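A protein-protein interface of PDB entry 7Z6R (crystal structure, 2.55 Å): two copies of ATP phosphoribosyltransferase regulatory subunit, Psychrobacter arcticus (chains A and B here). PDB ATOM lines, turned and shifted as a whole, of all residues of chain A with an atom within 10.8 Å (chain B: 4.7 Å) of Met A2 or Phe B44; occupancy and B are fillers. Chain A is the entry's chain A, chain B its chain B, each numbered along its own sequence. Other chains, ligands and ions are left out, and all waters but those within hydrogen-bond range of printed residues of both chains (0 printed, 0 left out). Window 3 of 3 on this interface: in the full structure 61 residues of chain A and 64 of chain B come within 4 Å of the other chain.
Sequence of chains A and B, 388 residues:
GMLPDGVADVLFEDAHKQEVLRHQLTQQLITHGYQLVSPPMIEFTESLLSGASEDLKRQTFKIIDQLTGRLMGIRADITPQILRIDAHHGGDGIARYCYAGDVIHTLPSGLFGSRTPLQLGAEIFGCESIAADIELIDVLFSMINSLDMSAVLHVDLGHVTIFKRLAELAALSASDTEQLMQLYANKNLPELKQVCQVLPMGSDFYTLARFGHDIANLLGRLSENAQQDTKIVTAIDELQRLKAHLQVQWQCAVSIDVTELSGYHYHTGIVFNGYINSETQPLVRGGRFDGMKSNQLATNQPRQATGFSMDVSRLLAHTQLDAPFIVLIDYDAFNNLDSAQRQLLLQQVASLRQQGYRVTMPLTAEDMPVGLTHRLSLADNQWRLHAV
Of chain B, only Phe B44 (3.3 Å) comes within 4 Å of Met A2.
No residue of chain A comes within 4 Å of Thr B45.
No residue of chain A comes within 4 Å of Glu B46.
No residue of chain A comes within 4 Å of Ser B47.
No residue of chain A comes within 4 Å of Leu B48.
Asp B65 touches one residue of chain A.
No residue of chain A comes within 4 Å of Arg B70.
Met B72 touches two residues of chain A.
Of the printed residues of chain B, Leu A3 touches Glu B43 and Phe B44.
Printed residues of chain B within 4 Å of Arg A115: Asp B65 (3.3 Å).
Leu B71 touches none of the printed residues of chain A.
Thr A106 touches none of the printed residues of chain B.
The nearest printed residue of chain B that does not touch Met A2 is Ser B47 (4.7 Å).
The nearest residue of chain A that does not touch Phe B44 is Asp A5 (5.2 Å).
No position is printed for both chains.
Phe B44 touches Met A2.
Glu B43 touches Leu A3.
Phe B44 touches Leu A3 (CE2 to C, 3.6 Å).
N of Pro A4 touches CE2 of Phe B44, at 3.4 Å.
Pro A4 touches Met B72.
Met B72 touches Phe A61 (CE to CZ, 3.8 Å).
The backbone carbonyl oxygen (O) of Gly A6 is in hydrogen-bond range of the backbone NH (N) of Arg A115 (2.6 Å).
O of Asp A5 is in hydrogen-bond range of NH2 of Arg A115, 2.8 Å away.
The backbone NH (N) of Asp B65 is in hydrogen-bond range of the backbone carbonyl oxygen (O) of Arg B70 (2.9 Å).
NH1 of Arg A115 sits at hydrogen-bond distance from O of Thr A106, at 2.8 Å.
O of Phe B44 is in hydrogen-bond range of OG of Ser B47 (3.2 Å).
The side-chain carboxylate of Glu B43 sits at hydrogen-bond distance from the backbone NH of Leu B48 (3.5 Å).
The guanidinium group (NH1) of Arg A115 lies within salt-bridge range of the side-chain carboxylate (OD1) of Asp B65, at 3.3 Å.
Hydrophobic or aromatic side chains of chain B that line the printed part of chain A: Phe B44 and Met B72.
Of the 12 printed residues of chain A, 5 touch a printed residue of chain B.
Printed residues of chain A that touch a printed residue of chain B: Met A2, Leu A3, Pro A4, Phe A61 and Arg A115.
Hydrophobic or aromatic side chains of chain A within 4 Å of the printed part of chain B: Leu A3, Pro A4 and Phe A61.
Among the printed residues, Asp or Glu carboxylates within 4 Å of a Lys or Arg side-chain nitrogen of the other chain: Arg A115 with Asp B65.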
ATOM      1  N   MET A   2      38.215  -9.753  15.218  1.00  0.00           N
ATOM      2  CA  MET A   2      37.387  -8.628  15.748  1.00  0.00           C
ATOM      3  C   MET A   2      36.053  -8.544  14.988  1.00  0.00           C
ATOM      4  O   MET A   2      35.025  -8.302  15.643  1.00  0.00           O
ATOM      5  CB  MET A   2      38.126  -7.286  15.631  1.00  0.00           C
ATOM      6  N   LEU A   3      36.057  -8.689  13.660  1.00  0.00           N
ATOM      7  CA  LEU A   3      34.827  -8.542  12.838  1.00  0.00           C
ATOM      8  C   LEU A   3      34.246  -9.929  12.588  1.00  0.00           C
ATOM      9  O   LEU A   3      34.985 -10.904  12.605  1.00  0.00           O
ATOM     10  CB  LEU A   3      35.139  -7.854  11.502  1.00  0.00           C
ATOM     11  CG  LEU A   3      35.693  -6.434  11.566  1.00  0.00           C
ATOM     12  CD1 LEU A   3      36.309  -6.052  10.229  1.00  0.00           C
ATOM     13  CD2 LEU A   3      34.603  -5.455  11.952  1.00  0.00           C
ATOM     14  N   PRO A   4      32.925 -10.044  12.314  1.00  0.00           N
ATOM     15  CA  PRO A   4      32.319 -11.319  11.945  1.00  0.00           C
ATOM     16  C   PRO A   4      32.915 -11.843  10.634  1.00  0.00           C
ATOM     17  O   PRO A   4      33.239 -11.025   9.777  1.00  0.00           O
ATOM     18  CB  PRO A   4      30.826 -11.003  11.753  1.00  0.00           C
ATOM     19  CG  PRO A   4      30.618  -9.650  12.419  1.00  0.00           C
ATOM     20  CD  PRO A   4      31.950  -8.943  12.309  1.00  0.00           C
ATOM     21  N   ASP A   5      33.036 -13.169  10.500  1.00  0.00           N
ATOM     22  CA  ASP A   5      33.462 -13.852   9.248  1.00  0.00           C
ATOM     23  C   ASP A   5      32.716 -13.215   8.070  1.00  0.00           C
ATOM     24  O   ASP A   5      31.508 -12.916   8.221  1.00  0.00           O
ATOM     25  N   GLY A   6      33.409 -12.992   6.954  1.00  0.00           N
ATOM     26  CA  GLY A   6      32.815 -12.445   5.716  1.00  0.00           C
ATOM     27  C   GLY A   6      32.512 -10.961   5.848  1.00  0.00           C
ATOM     28  O   GLY A   6      31.681 -10.447   5.075  1.00  0.00           O
ATOM     29  N   VAL A   7      33.136 -10.292   6.816  1.00  0.00           N
ATOM     30  CA  VAL A   7      32.977  -8.830   7.044  1.00  0.00           C
ATOM     31  C   VAL A   7      34.380  -8.255   7.226  1.00  0.00           C
ATOM     32  O   VAL A   7      35.092  -8.671   8.169  1.00  0.00           O
ATOM     33  CB  VAL A   7      32.058  -8.530   8.239  1.00  0.00           C
ATOM     34  CG1 VAL A   7      31.858  -7.042   8.447  1.00  0.00           C
ATOM     35  CG2 VAL A   7      30.713  -9.219   8.095  1.00  0.00           C
ATOM     36  N   ALA A   8      34.780  -7.378   6.312  1.00  0.00           N
ATOM     37  CA  ALA A   8      36.125  -6.768   6.314  1.00  0.00           C
ATOM     38  C   ALA A   8      36.003  -5.245   6.220  1.00  0.00           C
ATOM     39  O   ALA A   8      35.066  -4.759   5.570  1.00  0.00           O
ATOM     40  CB  ALA A   8      36.916  -7.350   5.179  1.00  0.00           C
ATOM     41  N   ASP A   9      36.920  -4.522   6.847  1.00  0.00           N
ATOM     42  CA  ASP A   9      37.193  -3.111   6.473  1.00  0.00           C
ATOM     43  C   ASP A   9      37.727  -3.103   5.037  1.00  0.00           C
ATOM     44  O   ASP A   9      38.375  -4.077   4.642  1.00  0.00           O
ATOM     45  CB  ASP A   9      38.168  -2.433   7.443  1.00  0.00           C
ATOM     46  CG  ASP A   9      37.544  -2.109   8.790  1.00  0.00           C
ATOM     47  OD1 ASP A   9      36.367  -1.700   8.811  1.00  0.00           O
ATOM     48  OD2 ASP A   9      38.237  -2.274   9.823  1.00  0.00           O
ATOM     49  N   PHE A  61      18.487 -10.523   6.494  1.00  0.00           N
ATOM     50  CA  PHE A  61      18.290 -10.107   7.904  1.00  0.00           C
ATOM     51  C   PHE A  61      16.926  -9.437   8.044  1.00  0.00           C
ATOM     52  O   PHE A  61      16.646  -8.504   7.282  1.00  0.00           O
ATOM     53  CB  PHE A  61      19.394  -9.146   8.360  1.00  0.00           C
ATOM     54  CG  PHE A  61      20.709  -9.819   8.658  1.00  0.00           C
ATOM     55  CD1 PHE A  61      20.846 -10.627   9.780  1.00  0.00           C
ATOM     56  CD2 PHE A  61      21.795  -9.663   7.810  1.00  0.00           C
ATOM     57  CE1 PHE A  61      22.046 -11.261  10.046  1.00  0.00           C
ATOM     58  CE2 PHE A  61      22.992 -10.308   8.075  1.00  0.00           C
ATOM     59  CZ  PHE A  61      23.113 -11.104   9.192  1.00  0.00           C
ATOM     60  N   THR A 106      23.077 -12.905   5.517  1.00  0.00           N
ATOM     61  CA  THR A 106      23.079 -13.606   6.832  1.00  0.00           C
ATOM     62  C   THR A 106      24.254 -14.587   6.876  1.00  0.00           C
ATOM     63  O   THR A 106      24.993 -14.567   7.867  1.00  0.00           O
ATOM     64  CB  THR A 106      21.735 -14.285   7.119  1.00  0.00           C
ATOM     65  OG1 THR A 106      21.454 -15.216   6.081  1.00  0.00           O
ATOM     66  CG2 THR A 106      20.589 -13.309   7.227  1.00  0.00           C
ATOM     67  N   ARG A 115      29.985 -11.261   3.220  1.00  0.00           N
ATOM     68  CA  ARG A 115      28.573 -11.026   3.625  1.00  0.00           C
ATOM     69  C   ARG A 115      28.188  -9.556   3.407  1.00  0.00           C
ATOM     70  O   ARG A 115      27.046  -9.202   3.731  1.00  0.00           O
ATOM     71  CB  ARG A 115      28.394 -11.415   5.098  1.00  0.00           C
ATOM     72  CG  ARG A 115      28.357 -12.919   5.316  1.00  0.00           C
ATOM     73  CD  ARG A 115      27.776 -13.293   6.658  1.00  0.00           C
ATOM     74  NE  ARG A 115      28.758 -13.319   7.724  1.00  0.00           N
ATOM     75  CZ  ARG A 115      28.450 -13.485   9.001  1.00  0.00           C
ATOM     76  NH1 ARG A 115      27.190 -13.612   9.375  1.00  0.00           N
ATOM     77  NH2 ARG A 115      29.398 -13.511   9.910  1.00  0.00           N
ATOM     78  N   THR A 116      29.104  -8.735   2.894  1.00  0.00           N
ATOM     79  CA  THR A 116      28.904  -7.271   2.702  1.00  0.00           C
ATOM     80  C   THR A 116      29.355  -6.878   1.302  1.00  0.00           C
ATOM     81  O   THR A 116      30.131  -5.939   1.131  1.00  0.00           O
ATOM     82  CB  THR A 116      29.641  -6.468   3.782  1.00  0.00           C
ATOM     83  OG1 THR A 116      30.981  -6.964   3.849  1.00  0.00           O
ATOM     84  CG2 THR A 116      28.966  -6.548   5.131  1.00  0.00           C
ATOM     85  N   GLU B  43      28.837  -5.118  12.316  1.00  0.00           N
ATOM     86  CA  GLU B  43      29.899  -5.559  13.253  1.00  0.00           C
ATOM     87  C   GLU B  43      29.207  -6.242  14.426  1.00  0.00           C
ATOM     88  O   GLU B  43      28.001  -5.997  14.637  1.00  0.00           O
ATOM     89  CB  GLU B  43      30.687  -4.373  13.834  1.00  0.00           C
ATOM     90  CG  GLU B  43      31.709  -3.780  12.892  1.00  0.00           C
ATOM     91  CD  GLU B  43      32.545  -2.664  13.507  1.00  0.00           C
ATOM     92  OE1 GLU B  43      32.713  -2.635  14.743  1.00  0.00           O
ATOM     93  OE2 GLU B  43      33.037  -1.812  12.744  1.00  0.00           O
ATOM     94  N   PHE B  44      29.963  -7.007  15.198  1.00  0.00           N
ATOM     95  CA  PHE B  44      29.557  -7.422  16.562  1.00  0.00           C
ATOM     96  C   PHE B  44      29.330  -6.139  17.360  1.00  0.00           C
ATOM     97  O   PHE B  44      30.088  -5.166  17.141  1.00  0.00           O
ATOM     98  CB  PHE B  44      30.632  -8.300  17.199  1.00  0.00           C
ATOM     99  CG  PHE B  44      30.887  -9.607  16.504  1.00  0.00           C
ATOM    100  CD1 PHE B  44      29.856 -10.501  16.278  1.00  0.00           C
ATOM    101  CD2 PHE B  44      32.163  -9.953  16.100  1.00  0.00           C
ATOM    102  CE1 PHE B  44      30.100 -11.717  15.653  1.00  0.00           C
ATOM    103  CE2 PHE B  44      32.406 -11.164  15.476  1.00  0.00           C
ATOM    104  CZ  PHE B  44      31.377 -12.050  15.263  1.00  0.00           C
ATOM    105  N   THR B  45      28.328  -6.132  18.246  1.00  0.00           N
ATOM    106  CA  THR B  45      27.984  -4.988  19.138  1.00  0.00           C
ATOM    107  C   THR B  45      29.157  -4.682  20.079  1.00  0.00           C
ATOM    108  O   THR B  45      29.305  -3.493  20.446  1.00  0.00           O
ATOM    109  CB  THR B  45      26.683  -5.248  19.908  1.00  0.00           C
ATOM    110  OG1 THR B  45      26.719  -6.587  20.401  1.00  0.00           O
ATOM    111  CG2 THR B  45      25.442  -5.081  19.058  1.00  0.00           C
ATOM    112  N   GLU B  46      29.961  -5.694  20.440  1.00  0.00           N
ATOM    113  CA  GLU B  46      31.128  -5.538  21.355  1.00  0.00           C
ATOM    114  C   GLU B  46      31.984  -4.375  20.829  1.00  0.00           C
ATOM    115  O   GLU B  46      32.271  -3.458  21.626  1.00  0.00           O
ATOM    116  CB  GLU B  46      31.919  -6.847  21.491  1.00  0.00           C
ATOM    117  N   SER B  47      32.316  -4.377  19.529  1.00  0.00           N
ATOM    118  CA  SER B  47      33.148  -3.337  18.860  1.00  0.00           C
ATOM    119  C   SER B  47      32.300  -2.126  18.440  1.00  0.00           C
ATOM    120  O   SER B  47      32.732  -0.983  18.711  1.00  0.00           O
ATOM    121  CB  SER B  47      33.900  -3.907  17.687  1.00  0.00           C
ATOM    122  OG  SER B  47      33.034  -4.113  16.578  1.00  0.00           O
ATOM    123  N   LEU B  48      31.140  -2.359  17.818  1.00  0.00           N
ATOM    124  CA  LEU B  48      30.309  -1.310  17.173  1.00  0.00           C
ATOM    125  C   LEU B  48      29.789  -0.307  18.202  1.00  0.00           C
ATOM    126  O   LEU B  48      29.550   0.837  17.806  1.00  0.00           O
ATOM    127  CB  LEU B  48      29.128  -1.972  16.458  1.00  0.00           C
ATOM    128  CG  LEU B  48      28.287  -1.057  15.565  1.00  0.00           C
ATOM    129  CD1 LEU B  48      29.117  -0.528  14.401  1.00  0.00           C
ATOM    130  CD2 LEU B  48      27.055  -1.789  15.044  1.00  0.00           C
ATOM    131  N   ASP B  65      24.309 -13.011  14.422  1.00  0.00           N
ATOM    132  CA  ASP B  65      25.303 -13.735  13.588  1.00  0.00           C
ATOM    133  C   ASP B  65      24.972 -15.223  13.648  1.00  0.00           C
ATOM    134  O   ASP B  65      25.190 -15.822  14.711  1.00  0.00           O
ATOM    135  CB  ASP B  65      26.737 -13.490  14.065  1.00  0.00           C
ATOM    136  CG  ASP B  65      27.795 -14.243  13.268  1.00  0.00           C
ATOM    137  OD1 ASP B  65      27.413 -14.968  12.360  1.00  0.00           O
ATOM    138  OD2 ASP B  65      28.998 -14.104  13.564  1.00  0.00           O
ATOM    139  N   THR B  68      27.977 -17.784  14.607  1.00  0.00           N
ATOM    140  CA  THR B  68      28.554 -17.818  15.984  1.00  0.00           C
ATOM    141  C   THR B  68      27.483 -17.670  17.078  1.00  0.00           C
ATOM    142  O   THR B  68      27.818 -17.884  18.251  1.00  0.00           O
ATOM    143  CB  THR B  68      29.595 -16.697  16.153  1.00  0.00           C
ATOM    144  OG1 THR B  68      28.924 -15.441  16.033  1.00  0.00           O
ATOM    145  CG2 THR B  68      30.728 -16.792  15.152  1.00  0.00           C
ATOM    146  N   ARG B  70      26.399 -14.858  18.072  1.00  0.00           N
ATOM    147  CA  ARG B  70      26.726 -13.584  18.776  1.00  0.00           C
ATOM    148  C   ARG B  70      25.894 -12.429  18.201  1.00  0.00           C
ATOM    149  O   ARG B  70      25.558 -12.477  16.993  1.00  0.00           O
ATOM    150  CB  ARG B  70      28.211 -13.253  18.622  1.00  0.00           C
ATOM    151  CG  ARG B  70      29.162 -14.281  19.212  1.00  0.00           C
ATOM    152  CD  ARG B  70      30.619 -13.851  19.137  1.00  0.00           C
ATOM    153  NE  ARG B  70      30.823 -12.472  19.583  1.00  0.00           N
ATOM    154  CZ  ARG B  70      31.901 -11.720  19.325  1.00  0.00           C
ATOM    155  NH1 ARG B  70      32.910 -12.216  18.626  1.00  0.00           N
ATOM    156  NH2 ARG B  70      31.969 -10.478  19.780  1.00  0.00           N
ATOM    157  N   LEU B  71      25.591 -11.427  19.025  1.00  0.00           N
ATOM    158  CA  LEU B  71      24.836 -10.209  18.633  1.00  0.00           C
ATOM    159  C   LEU B  71      25.684  -9.321  17.715  1.00  0.00           C
ATOM    160  O   LEU B  71      26.868  -9.050  18.062  1.00  0.00           O
ATOM    161  CB  LEU B  71      24.471  -9.424  19.893  1.00  0.00           C
ATOM    162  CG  LEU B  71      23.524  -8.254  19.659  1.00  0.00           C
ATOM    163  CD1 LEU B  71      22.182  -8.757  19.141  1.00  0.00           C
ATOM    164  CD2 LEU B  71      23.352  -7.425  20.927  1.00  0.00           C
ATOM    165  N   MET B  72      25.097  -8.877  16.599  1.00  0.00           N
ATOM    166  CA  MET B  72      25.682  -7.869  15.676  1.00  0.00           C
ATOM    167  C   MET B  72      24.724  -6.678  15.608  1.00  0.00           C
ATOM    168  O   MET B  72      23.570  -6.804  16.101  1.00  0.00           O
ATOM    169  CB  MET B  72      25.886  -8.420  14.261  1.00  0.00           C
ATOM    170  CG  MET B  72      26.935  -9.501  14.177  1.00  0.00           C
ATOM    171  SD  MET B  72      27.211 -10.098  12.505  1.00  0.00           S
ATOM    172  CE  MET B  72      25.546 -10.589  12.042  1.00  0.00           C
